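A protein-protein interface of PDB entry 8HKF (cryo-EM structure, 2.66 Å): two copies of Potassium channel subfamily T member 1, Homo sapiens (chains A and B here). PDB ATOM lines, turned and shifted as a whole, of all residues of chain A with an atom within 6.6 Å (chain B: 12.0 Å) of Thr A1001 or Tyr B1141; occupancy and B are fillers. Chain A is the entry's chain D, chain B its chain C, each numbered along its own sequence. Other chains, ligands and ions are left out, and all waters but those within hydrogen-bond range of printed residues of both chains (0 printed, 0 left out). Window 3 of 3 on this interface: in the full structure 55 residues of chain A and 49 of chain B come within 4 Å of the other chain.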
ATOM      1  N   LYS A 604       1.402  -8.919  12.910  1.00  0.00           N
ATOM      2  CA  LYS A 604       0.818 -10.039  12.188  1.00  0.00           C
ATOM      3  C   LYS A 604       1.859 -10.869  11.451  1.00  0.00           C
ATOM      4  O   LYS A 604       1.496 -11.824  10.758  1.00  0.00           O
ATOM      5  CB  LYS A 604      -0.233  -9.536  11.194  1.00  0.00           C
ATOM      6  CG  LYS A 604       0.338  -8.655  10.093  1.00  0.00           C
ATOM      7  CD  LYS A 604      -0.744  -8.207   9.124  1.00  0.00           C
ATOM      8  CE  LYS A 604      -0.166  -7.326   8.026  1.00  0.00           C
ATOM      9  NZ  LYS A 604      -1.206  -6.871   7.062  1.00  0.00           N
ATOM     10  N   SER A 605       3.138 -10.532  11.586  1.00  0.00           N
ATOM     11  CA  SER A 605       4.197 -11.185  10.832  1.00  0.00           C
ATOM     12  C   SER A 605       4.738 -12.379  11.606  1.00  0.00           C
ATOM     13  O   SER A 605       5.052 -12.269  12.796  1.00  0.00           O
ATOM     14  CB  SER A 605       5.326 -10.200  10.533  1.00  0.00           C
ATOM     15  OG  SER A 605       5.954  -9.770  11.727  1.00  0.00           O
ATOM     16  N   ILE A 606       4.844 -13.514  10.925  1.00  0.00           N
ATOM     17  CA  ILE A 606       5.452 -14.712  11.489  1.00  0.00           C
ATOM     18  C   ILE A 606       6.945 -14.670  11.208  1.00  0.00           C
ATOM     19  O   ILE A 606       7.366 -14.435  10.069  1.00  0.00           O
ATOM     20  CB  ILE A 606       4.818 -15.982  10.901  1.00  0.00           C
ATOM     21  CG1 ILE A 606       3.325 -16.028  11.213  1.00  0.00           C
ATOM     22  CG2 ILE A 606       5.519 -17.217  11.435  1.00  0.00           C
ATOM     23  CD1 ILE A 606       2.559 -16.986  10.337  1.00  0.00           C
ATOM     24  N   LEU A 607       7.748 -14.888  12.242  1.00  0.00           N
ATOM     25  CA  LEU A 607       9.199 -14.854  12.134  1.00  0.00           C
ATOM     26  C   LEU A 607       9.754 -16.252  12.357  1.00  0.00           C
ATOM     27  O   LEU A 607       9.499 -16.863  13.399  1.00  0.00           O
ATOM     28  CB  LEU A 607       9.803 -13.884  13.149  1.00  0.00           C
ATOM     29  CG  LEU A 607       9.740 -12.388  12.832  1.00  0.00           C
ATOM     30  CD1 LEU A 607       8.358 -11.826  13.122  1.00  0.00           C
ATOM     31  CD2 LEU A 607      10.798 -11.643  13.624  1.00  0.00           C
ATOM     32  N   PRO A 764      11.142  -8.020  -2.225  1.00  0.00           N
ATOM     33  CA  PRO A 764      12.507  -7.582  -2.528  1.00  0.00           C
ATOM     34  C   PRO A 764      13.519  -8.289  -1.643  1.00  0.00           C
ATOM     35  O   PRO A 764      13.553  -8.088  -0.428  1.00  0.00           O
ATOM     36  CB  PRO A 764      12.454  -6.075  -2.259  1.00  0.00           C
ATOM     37  CG  PRO A 764      11.438  -5.947  -1.119  1.00  0.00           C
ATOM     38  CD  PRO A 764      10.625  -7.272  -1.074  1.00  0.00           C
ATOM     39  N   THR A 990       2.089 -19.018   4.757  1.00  0.00           N
ATOM     40  CA  THR A 990       3.123 -18.076   5.177  1.00  0.00           C
ATOM     41  C   THR A 990       4.400 -18.802   5.582  1.00  0.00           C
ATOM     42  O   THR A 990       5.508 -18.368   5.245  1.00  0.00           O
ATOM     43  CB  THR A 990       2.607 -17.216   6.331  1.00  0.00           C
ATOM     44  OG1 THR A 990       1.372 -16.599   5.953  1.00  0.00           O
ATOM     45  CG2 THR A 990       3.616 -16.136   6.676  1.00  0.00           C
ATOM     46  N   LEU A 994       8.086 -18.441   3.807  1.00  0.00           N
ATOM     47  CA  LEU A 994       9.225 -18.033   4.621  1.00  0.00           C
ATOM     48  C   LEU A 994      10.384 -19.010   4.473  1.00  0.00           C
ATOM     49  O   LEU A 994      11.548 -18.597   4.419  1.00  0.00           O
ATOM     50  CB  LEU A 994       8.811 -17.914   6.087  1.00  0.00           C
ATOM     51  CG  LEU A 994       7.962 -16.714   6.505  1.00  0.00           C
ATOM     52  CD1 LEU A 994       7.393 -16.944   7.892  1.00  0.00           C
ATOM     53  CD2 LEU A 994       8.784 -15.441   6.473  1.00  0.00           C
ATOM     54  N   ASP A 999       8.457 -14.785   0.720  1.00  0.00           N
ATOM     55  CA  ASP A 999       8.169 -13.555   1.443  1.00  0.00           C
ATOM     56  C   ASP A 999       9.293 -13.293   2.435  1.00  0.00           C
ATOM     57  O   ASP A 999       9.743 -14.209   3.130  1.00  0.00           O
ATOM     58  CB  ASP A 999       6.806 -13.611   2.145  1.00  0.00           C
ATOM     59  CG  ASP A 999       6.664 -14.797   3.081  1.00  0.00           C
ATOM     60  OD1 ASP A 999       7.550 -15.673   3.095  1.00  0.00           O
ATOM     61  OD2 ASP A 999       5.649 -14.851   3.806  1.00  0.00           O
ATOM     62  N   THR A1000       9.763 -12.052   2.472  1.00  0.00           N
ATOM     63  CA  THR A1000      10.921 -11.668   3.274  1.00  0.00           C
ATOM     64  C   THR A1000      10.458 -10.706   4.360  1.00  0.00           C
ATOM     65  O   THR A1000      10.230  -9.521   4.096  1.00  0.00           O
ATOM     66  CB  THR A1000      12.005 -11.040   2.403  1.00  0.00           C
ATOM     67  OG1 THR A1000      11.650  -9.686   2.099  1.00  0.00           O
ATOM     68  CG2 THR A1000      12.161 -11.819   1.107  1.00  0.00           C
ATOM     69  N   THR A1001      10.316 -11.215   5.568  1.00  0.00           N
ATOM     70  CA  THR A1001       9.998 -10.376   6.711  1.00  0.00           C
ATOM     71  C   THR A1001      11.271 -10.044   7.466  1.00  0.00           C
ATOM     72  O   THR A1001      12.049 -10.957   7.779  1.00  0.00           O
ATOM     73  CB  THR A1001       9.016 -11.078   7.643  1.00  0.00           C
ATOM     74  OG1 THR A1001       8.000 -11.725   6.867  1.00  0.00           O
ATOM     75  CG2 THR A1001       8.367 -10.073   8.576  1.00  0.00           C
ATOM     76  N   PRO A1002      11.536  -8.770   7.753  1.00  0.00           N
ATOM     77  CA  PRO A1002      12.744  -8.424   8.514  1.00  0.00           C
ATOM     78  C   PRO A1002      12.759  -9.121   9.866  1.00  0.00           C
ATOM     79  O   PRO A1002      11.793  -9.059  10.630  1.00  0.00           O
ATOM     80  CB  PRO A1002      12.644  -6.902   8.657  1.00  0.00           C
ATOM     81  CG  PRO A1002      11.800  -6.476   7.504  1.00  0.00           C
ATOM     82  CD  PRO A1002      10.798  -7.575   7.314  1.00  0.00           C
ATOM     83  N   GLY A1003      13.872  -9.786  10.157  1.00  0.00           N
ATOM     84  CA  GLY A1003      14.004 -10.570  11.364  1.00  0.00           C
ATOM     85  C   GLY A1003      13.597 -12.021  11.245  1.00  0.00           C
ATOM     86  O   GLY A1003      13.610 -12.731  12.257  1.00  0.00           O
ATOM     87  N   SER A1004      13.235 -12.482  10.053  1.00  0.00           N
ATOM     88  CA  SER A1004      12.843 -13.864   9.826  1.00  0.00           C
ATOM     89  C   SER A1004      14.009 -14.631   9.221  1.00  0.00           C
ATOM     90  O   SER A1004      14.731 -14.111   8.364  1.00  0.00           O
ATOM     91  CB  SER A1004      11.624 -13.949   8.906  1.00  0.00           C
ATOM     92  OG  SER A1004      11.273 -15.296   8.645  1.00  0.00           O
ATOM     93  N   GLY A1005      14.187 -15.871   9.668  1.00  0.00           N
ATOM     94  CA  GLY A1005      15.299 -16.683   9.231  1.00  0.00           C
ATOM     95  C   GLY A1005      15.103 -17.271   7.849  1.00  0.00           C
ATOM     96  O   GLY A1005      14.076 -17.095   7.195  1.00  0.00           O
ATOM     97  N   ASP A1202      18.126 -14.226  11.022  1.00  0.00           N
ATOM     98  CA  ASP A1202      18.414 -13.171  10.063  1.00  0.00           C
ATOM     99  C   ASP A1202      19.741 -12.498  10.401  1.00  0.00           C
ATOM    100  O   ASP A1202      19.912 -12.004  11.524  1.00  0.00           O
ATOM    101  CB  ASP A1202      17.288 -12.140  10.059  1.00  0.00           C
ATOM    102  CG  ASP A1202      17.281 -11.289   8.808  1.00  0.00           C
ATOM    103  OD1 ASP A1202      18.099 -10.349   8.726  1.00  0.00           O
ATOM    104  OD2 ASP A1202      16.459 -11.559   7.909  1.00  0.00           O
ATOM    105  N   TRP B1132      22.788   1.016   6.515  1.00  0.00           N
ATOM    106  CA  TRP B1132      22.044   1.519   5.365  1.00  0.00           C
ATOM    107  C   TRP B1132      21.236   0.414   4.698  1.00  0.00           C
ATOM    108  O   TRP B1132      20.129   0.664   4.205  1.00  0.00           O
ATOM    109  CB  TRP B1132      22.997   2.162   4.359  1.00  0.00           C
ATOM    110  N   ILE B1133      21.773  -0.808   4.664  1.00  0.00           N
ATOM    111  CA  ILE B1133      21.032  -1.936   4.105  1.00  0.00           C
ATOM    112  C   ILE B1133      19.775  -2.199   4.924  1.00  0.00           C
ATOM    113  O   ILE B1133      18.690  -2.432   4.376  1.00  0.00           O
ATOM    114  CB  ILE B1133      21.930  -3.184   4.033  1.00  0.00           C
ATOM    115  CG1 ILE B1133      23.084  -2.958   3.051  1.00  0.00           C
ATOM    116  CG2 ILE B1133      21.117  -4.411   3.647  1.00  0.00           C
ATOM    117  CD1 ILE B1133      22.693  -3.108   1.597  1.00  0.00           C
ATOM    118  N   SER B1134      19.903  -2.161   6.252  1.00  0.00           N
ATOM    119  CA  SER B1134      18.744  -2.351   7.118  1.00  0.00           C
ATOM    120  C   SER B1134      17.730  -1.229   6.939  1.00  0.00           C
ATOM    121  O   SER B1134      16.518  -1.470   6.961  1.00  0.00           O
ATOM    122  CB  SER B1134      19.187  -2.448   8.577  1.00  0.00           C
ATOM    123  OG  SER B1134      19.979  -3.601   8.794  1.00  0.00           O
ATOM    124  N   GLN B1135      18.208   0.008   6.770  1.00  0.00           N
ATOM    125  CA  GLN B1135      17.301   1.134   6.566  1.00  0.00           C
ATOM    126  C   GLN B1135      16.489   0.960   5.288  1.00  0.00           C
ATOM    127  O   GLN B1135      15.276   1.197   5.273  1.00  0.00           O
ATOM    128  CB  GLN B1135      18.093   2.442   6.532  1.00  0.00           C
ATOM    129  N   GLN B1136      17.146   0.547   4.203  1.00  0.00           N
ATOM    130  CA  GLN B1136      16.419   0.278   2.968  1.00  0.00           C
ATOM    131  C   GLN B1136      15.530  -0.948   3.109  1.00  0.00           C
ATOM    132  O   GLN B1136      14.425  -0.976   2.564  1.00  0.00           O
ATOM    133  CB  GLN B1136      17.393   0.103   1.803  1.00  0.00           C
ATOM    134  CG  GLN B1136      17.872   1.410   1.192  1.00  0.00           C
ATOM    135  CD  GLN B1136      19.029   1.216   0.233  1.00  0.00           C
ATOM    136  OE1 GLN B1136      19.203   0.140  -0.339  1.00  0.00           O
ATOM    137  NE2 GLN B1136      19.826   2.262   0.048  1.00  0.00           N
ATOM    138  N   ARG B1137      15.975  -1.957   3.856  1.00  0.00           N
ATOM    139  CA  ARG B1137      15.182  -3.173   4.009  1.00  0.00           C
ATOM    140  C   ARG B1137      13.839  -2.887   4.668  1.00  0.00           C
ATOM    141  O   ARG B1137      12.798  -3.384   4.223  1.00  0.00           O
ATOM    142  CB  ARG B1137      15.967  -4.205   4.817  1.00  0.00           C
ATOM    143  CG  ARG B1137      15.244  -5.524   4.989  1.00  0.00           C
ATOM    144  CD  ARG B1137      16.052  -6.480   5.838  1.00  0.00           C
ATOM    145  NE  ARG B1137      16.192  -5.977   7.198  1.00  0.00           N
ATOM    146  CZ  ARG B1137      17.107  -6.403   8.058  1.00  0.00           C
ATOM    147  NH1 ARG B1137      17.969  -7.352   7.732  1.00  0.00           N
ATOM    148  NH2 ARG B1137      17.166  -5.853   9.267  1.00  0.00           N
ATOM    149  N   LEU B1138      13.844  -2.088   5.737  1.00  0.00           N
ATOM    150  CA  LEU B1138      12.590  -1.730   6.391  1.00  0.00           C
ATOM    151  C   LEU B1138      11.731  -0.854   5.487  1.00  0.00           C
ATOM    152  O   LEU B1138      10.498  -0.946   5.509  1.00  0.00           O
ATOM    153  CB  LEU B1138      12.869  -1.024   7.718  1.00  0.00           C
ATOM    154  CG  LEU B1138      12.739  -1.859   8.994  1.00  0.00           C
ATOM    155  CD1 LEU B1138      11.357  -2.489   9.079  1.00  0.00           C
ATOM    156  CD2 LEU B1138      13.829  -2.920   9.089  1.00  0.00           C
ATOM    157  N   SER B1139      12.366   0.009   4.691  1.00  0.00           N
ATOM    158  CA  SER B1139      11.617   0.888   3.800  1.00  0.00           C
ATOM    159  C   SER B1139      10.892   0.092   2.721  1.00  0.00           C
ATOM    160  O   SER B1139       9.705   0.318   2.458  1.00  0.00           O
ATOM    161  CB  SER B1139      12.556   1.918   3.172  1.00  0.00           C
ATOM    162  OG  SER B1139      11.901   2.649   2.150  1.00  0.00           O
ATOM    163  N   LEU B1140      11.591  -0.853   2.085  1.00  0.00           N
ATOM    164  CA  LEU B1140      10.957  -1.649   1.040  1.00  0.00           C
ATOM    165  C   LEU B1140       9.925  -2.611   1.614  1.00  0.00           C
ATOM    166  O   LEU B1140       9.001  -3.022   0.903  1.00  0.00           O
ATOM    167  CB  LEU B1140      12.010  -2.413   0.236  1.00  0.00           C
ATOM    168  CG  LEU B1140      12.831  -1.571  -0.748  1.00  0.00           C
ATOM    169  CD1 LEU B1140      14.207  -1.255  -0.234  1.00  0.00           C
ATOM    170  CD2 LEU B1140      12.935  -2.252  -2.098  1.00  0.00           C
ATOM    171  N   TYR B1141      10.065  -2.982   2.887  1.00  0.00           N
ATOM    172  CA  TYR B1141       9.058  -3.819   3.526  1.00  0.00           C
ATOM    173  C   TYR B1141       7.797  -3.025   3.841  1.00  0.00           C
ATOM    174  O   TYR B1141       6.683  -3.546   3.717  1.00  0.00           O
ATOM    175  CB  TYR B1141       9.628  -4.446   4.797  1.00  0.00           C
ATOM    176  CG  TYR B1141       8.630  -5.271   5.574  1.00  0.00           C
ATOM    177  CD1 TYR B1141       8.162  -6.479   5.074  1.00  0.00           C
ATOM    178  CD2 TYR B1141       8.160  -4.846   6.810  1.00  0.00           C
ATOM    179  CE1 TYR B1141       7.251  -7.238   5.780  1.00  0.00           C
ATOM    180  CE2 TYR B1141       7.250  -5.599   7.523  1.00  0.00           C
ATOM    181  CZ  TYR B1141       6.799  -6.794   7.004  1.00  0.00           C
ATOM    182  OH  TYR B1141       5.892  -7.549   7.711  1.00  0.00           O
ATOM    183  N   ARG B1142       7.955  -1.764   4.243  1.00  0.00           N
ATOM    184  CA  ARG B1142       6.827  -0.917   4.603  1.00  0.00           C
ATOM    185  C   ARG B1142       6.118  -0.319   3.395  1.00  0.00           C
ATOM    186  O   ARG B1142       5.004   0.193   3.545  1.00  0.00           O
ATOM    187  CB  ARG B1142       7.296   0.217   5.517  1.00  0.00           C
ATOM    188  CG  ARG B1142       7.327  -0.128   6.994  1.00  0.00           C
ATOM    189  CD  ARG B1142       8.100   0.928   7.767  1.00  0.00           C
ATOM    190  NE  ARG B1142       8.292   0.567   9.166  1.00  0.00           N
ATOM    191  CZ  ARG B1142       9.254   1.053   9.938  1.00  0.00           C
ATOM    192  NH1 ARG B1142      10.135   1.925   9.477  1.00  0.00           N
ATOM    193  NH2 ARG B1142       9.333   0.654  11.204  1.00  0.00           N
ATOM    194  N   ARG B1143       6.731  -0.365   2.215  1.00  0.00           N
ATOM    195  CA  ARG B1143       6.165   0.302   1.052  1.00  0.00           C
ATOM    196  C   ARG B1143       4.894  -0.402   0.587  1.00  0.00           C
ATOM    197  O   ARG B1143       4.751  -1.623   0.696  1.00  0.00           O
ATOM    198  CB  ARG B1143       7.202   0.377  -0.071  1.00  0.00           C
ATOM    199  CG  ARG B1143       6.774   1.091  -1.341  1.00  0.00           C
ATOM    200  CD  ARG B1143       7.904   1.025  -2.355  1.00  0.00           C
ATOM    201  NE  ARG B1143       8.202  -0.328  -2.807  1.00  0.00           N
ATOM    202  CZ  ARG B1143       9.331  -0.686  -3.405  1.00  0.00           C
ATOM    203  NH1 ARG B1143      10.312   0.177  -3.600  1.00  0.00           N
ATOM    204  NH2 ARG B1143       9.475  -1.942  -3.822  1.00  0.00           N
ATOM    205  N   SER B1144       3.959   0.394   0.074  1.00  0.00           N
ATOM    206  CA  SER B1144       2.623  -0.079  -0.243  1.00  0.00           C
ATOM    207  C   SER B1144       2.552  -0.584  -1.682  1.00  0.00           C
ATOM    208  O   SER B1144       3.519  -0.521  -2.445  1.00  0.00           O
ATOM    209  CB  SER B1144       1.601   1.032  -0.009  1.00  0.00           C
ATOM    210  OG  SER B1144       2.021   2.240  -0.622  1.00  0.00           O
ATOM    211  N   GLU B1145       1.380  -1.103  -2.054  1.00  0.00           N
ATOM    212  CA  GLU B1145       1.165  -1.554  -3.423  1.00  0.00           C
ATOM    213  C   GLU B1145       1.073  -0.387  -4.397  1.00  0.00           C
ATOM    214  O   GLU B1145       1.488  -0.518  -5.553  1.00  0.00           O
ATOM    215  CB  GLU B1145      -0.098  -2.408  -3.505  1.00  0.00           C
ATOM    216  CG  GLU B1145      -0.238  -3.172  -4.809  1.00  0.00           C
ATOM    217  CD  GLU B1145      -1.336  -4.213  -4.759  1.00  0.00           C
ATOM    218  OE1 GLU B1145      -2.246  -4.080  -3.915  1.00  0.00           O
ATOM    219  OE2 GLU B1145      -1.288  -5.165  -5.567  1.00  0.00           O
ATOM    220  N   ARG B1146       0.533   0.751  -3.953  1.00  0.00           N
ATOM    221  CA  ARG B1146       0.487   1.924  -4.818  1.00  0.00           C
ATOM    222  C   ARG B1146       1.890   2.389  -5.179  1.00  0.00           C
ATOM    223  O   ARG B1146       2.145   2.794  -6.320  1.00  0.00           O
ATOM    224  CB  ARG B1146      -0.299   3.049  -4.144  1.00  0.00           C
ATOM    225  CG  ARG B1146      -0.288   4.355  -4.922  1.00  0.00           C
ATOM    226  CD  ARG B1146      -1.538   4.505  -5.779  1.00  0.00           C
ATOM    227  NE  ARG B1146      -1.572   3.540  -6.871  1.00  0.00           N
ATOM    228  CZ  ARG B1146      -0.977   3.710  -8.045  1.00  0.00           C
ATOM    229  NH1 ARG B1146      -0.290   4.807  -8.318  1.00  0.00           N
ATOM    230  NH2 ARG B1146      -1.074   2.756  -8.965  1.00  0.00           N
ATOM    231  N   GLN B1147       2.814   2.341  -4.218  1.00  0.00           N
ATOM    232  CA  GLN B1147       4.207   2.645  -4.521  1.00  0.00           C
ATOM    233  C   GLN B1147       4.797   1.617  -5.476  1.00  0.00           C
ATOM    234  O   GLN B1147       5.578   1.965  -6.369  1.00  0.00           O
ATOM    235  CB  GLN B1147       5.022   2.722  -3.231  1.00  0.00           C
ATOM    236  CG  GLN B1147       4.545   3.794  -2.269  1.00  0.00           C
ATOM    237  CD  GLN B1147       5.529   4.048  -1.147  1.00  0.00           C
ATOM    238  OE1 GLN B1147       6.740   3.925  -1.329  1.00  0.00           O
ATOM    239  NE2 GLN B1147       5.014   4.406   0.023  1.00  0.00           N
ATOM    240  N   GLU B1148       4.436   0.343  -5.306  1.00  0.00           N
ATOM    241  CA  GLU B1148       4.915  -0.694  -6.216  1.00  0.00           C
ATOM    242  C   GLU B1148       4.480  -0.408  -7.647  1.00  0.00           C
ATOM    243  O   GLU B1148       5.287  -0.473  -8.582  1.00  0.00           O
ATOM    244  CB  GLU B1148       4.393  -2.063  -5.776  1.00  0.00           C
ATOM    245  CG  GLU B1148       5.130  -2.686  -4.616  1.00  0.00           C
ATOM    246  CD  GLU B1148       4.627  -4.071  -4.281  1.00  0.00           C
ATOM    247  OE1 GLU B1148       3.692  -4.181  -3.465  1.00  0.00           O
ATOM    248  OE2 GLU B1148       5.160  -5.051  -4.844  1.00  0.00           O
ATOM    249  N   GLU B1151       6.337   2.818  -9.050  1.00  0.00           N
ATOM    250  CA  GLU B1151       7.726   2.609  -9.451  1.00  0.00           C
ATOM    251  C   GLU B1151       7.826   1.749 -10.704  1.00  0.00           C
ATOM    252  O   GLU B1151       8.729   1.955 -11.521  1.00  0.00           O
ATOM    253  CB  GLU B1151       8.535   1.974  -8.318  1.00  0.00           C
ATOM    254  CG  GLU B1151       8.452   2.679  -6.966  1.00  0.00           C
ATOM    255  CD  GLU B1151       8.234   4.177  -7.078  1.00  0.00           C
ATOM    256  OE1 GLU B1151       7.080   4.624  -6.906  1.00  0.00           O
ATOM    257  OE2 GLU B1151       9.215   4.910  -7.325  1.00  0.00           O
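NH1 of Arg B1137 lies within salt-bridge range of OD1 of Asp A1202 (3.2 Å).
Among the printed residues, merely in contact across the chains: Pro A1002 with Tyr B1141 (3.6 Å), Thr A1001 with Tyr B1141 (3.6 Å), Thr A1000 with Tyr B1141 (3.8 Å), Pro A764 with Leu B1140 (3.8 Å), Ser A605 with Tyr B1141 (3.9 Å) and Pro A1002 with Arg B1137 (3.9 Å).
Thr A1001 touches just one residue of chain B: Tyr B1141 (3.6 Å).
Tyr B1141 touches just these residues of chain A: Ser A605 (3.9 Å), Thr A1000 (3.8 Å), Thr A1001 (3.6 Å) and Pro A1002 (3.6 Å).
Of chain B, only Tyr B1141 (3.9 Å) comes within 4 Å of Ser A605.
Of the printed residues of chain B, Pro A764 touches Leu B1140 (3.8 Å).
No residue of chain B comes within 4 Å of Leu A994.
Thr A1000 touches just one residue of chain B: Tyr B1141 (3.8 Å).
Of the printed residues of chain B, Pro A1002 touches Arg B1137 and Tyr B1141.
Gly A1003 touches none of the printed residues of chain B.
No residue of chain B comes within 4 Å of Ser A1004.
Printed residues of chain A within 4 Å of Arg B1137: Pro A1002 (3.9 Å) and Asp A1202 (3.2 Å).
Of the printed residues of chain A, Leu B1140 touches Pro A764 (3.8 Å).
Of the printed residues of chain B, Asp A1202 touches Arg B1137.
Ser B1139 touches none of the printed residues of chain A.
The nearest residue of chain B that does not touch Thr A1001 is Arg B1137 (6.2 Å).
The nearest residue of chain A that does not touch Tyr B1141 is Pro A764 (5.2 Å).
Of the 15 printed residues of chain A, 6 touch a printed residue of chain B.
Printed residues of chain A that touch a printed residue of chain B: Ser A605, Pro A764, Thr A1000, Thr A1001, Pro A1002 and Asp A1202.
Hydrophobic or aromatic side chains of chain A within 4 Å of the printed part of chain B: Pro A764 and Pro A1002.
Of the 18 printed residues of chain B, 3 touch a printed residue of chain A.
Hydrophobic or aromatic side chains of chain B that line the printed part of chain A: Leu B1140 and Tyr B1141.
No position is printed for both chains.
Of the 7 pairs that touch across the chains among the printed residues, none has its exchanged pair printed and touching as well.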
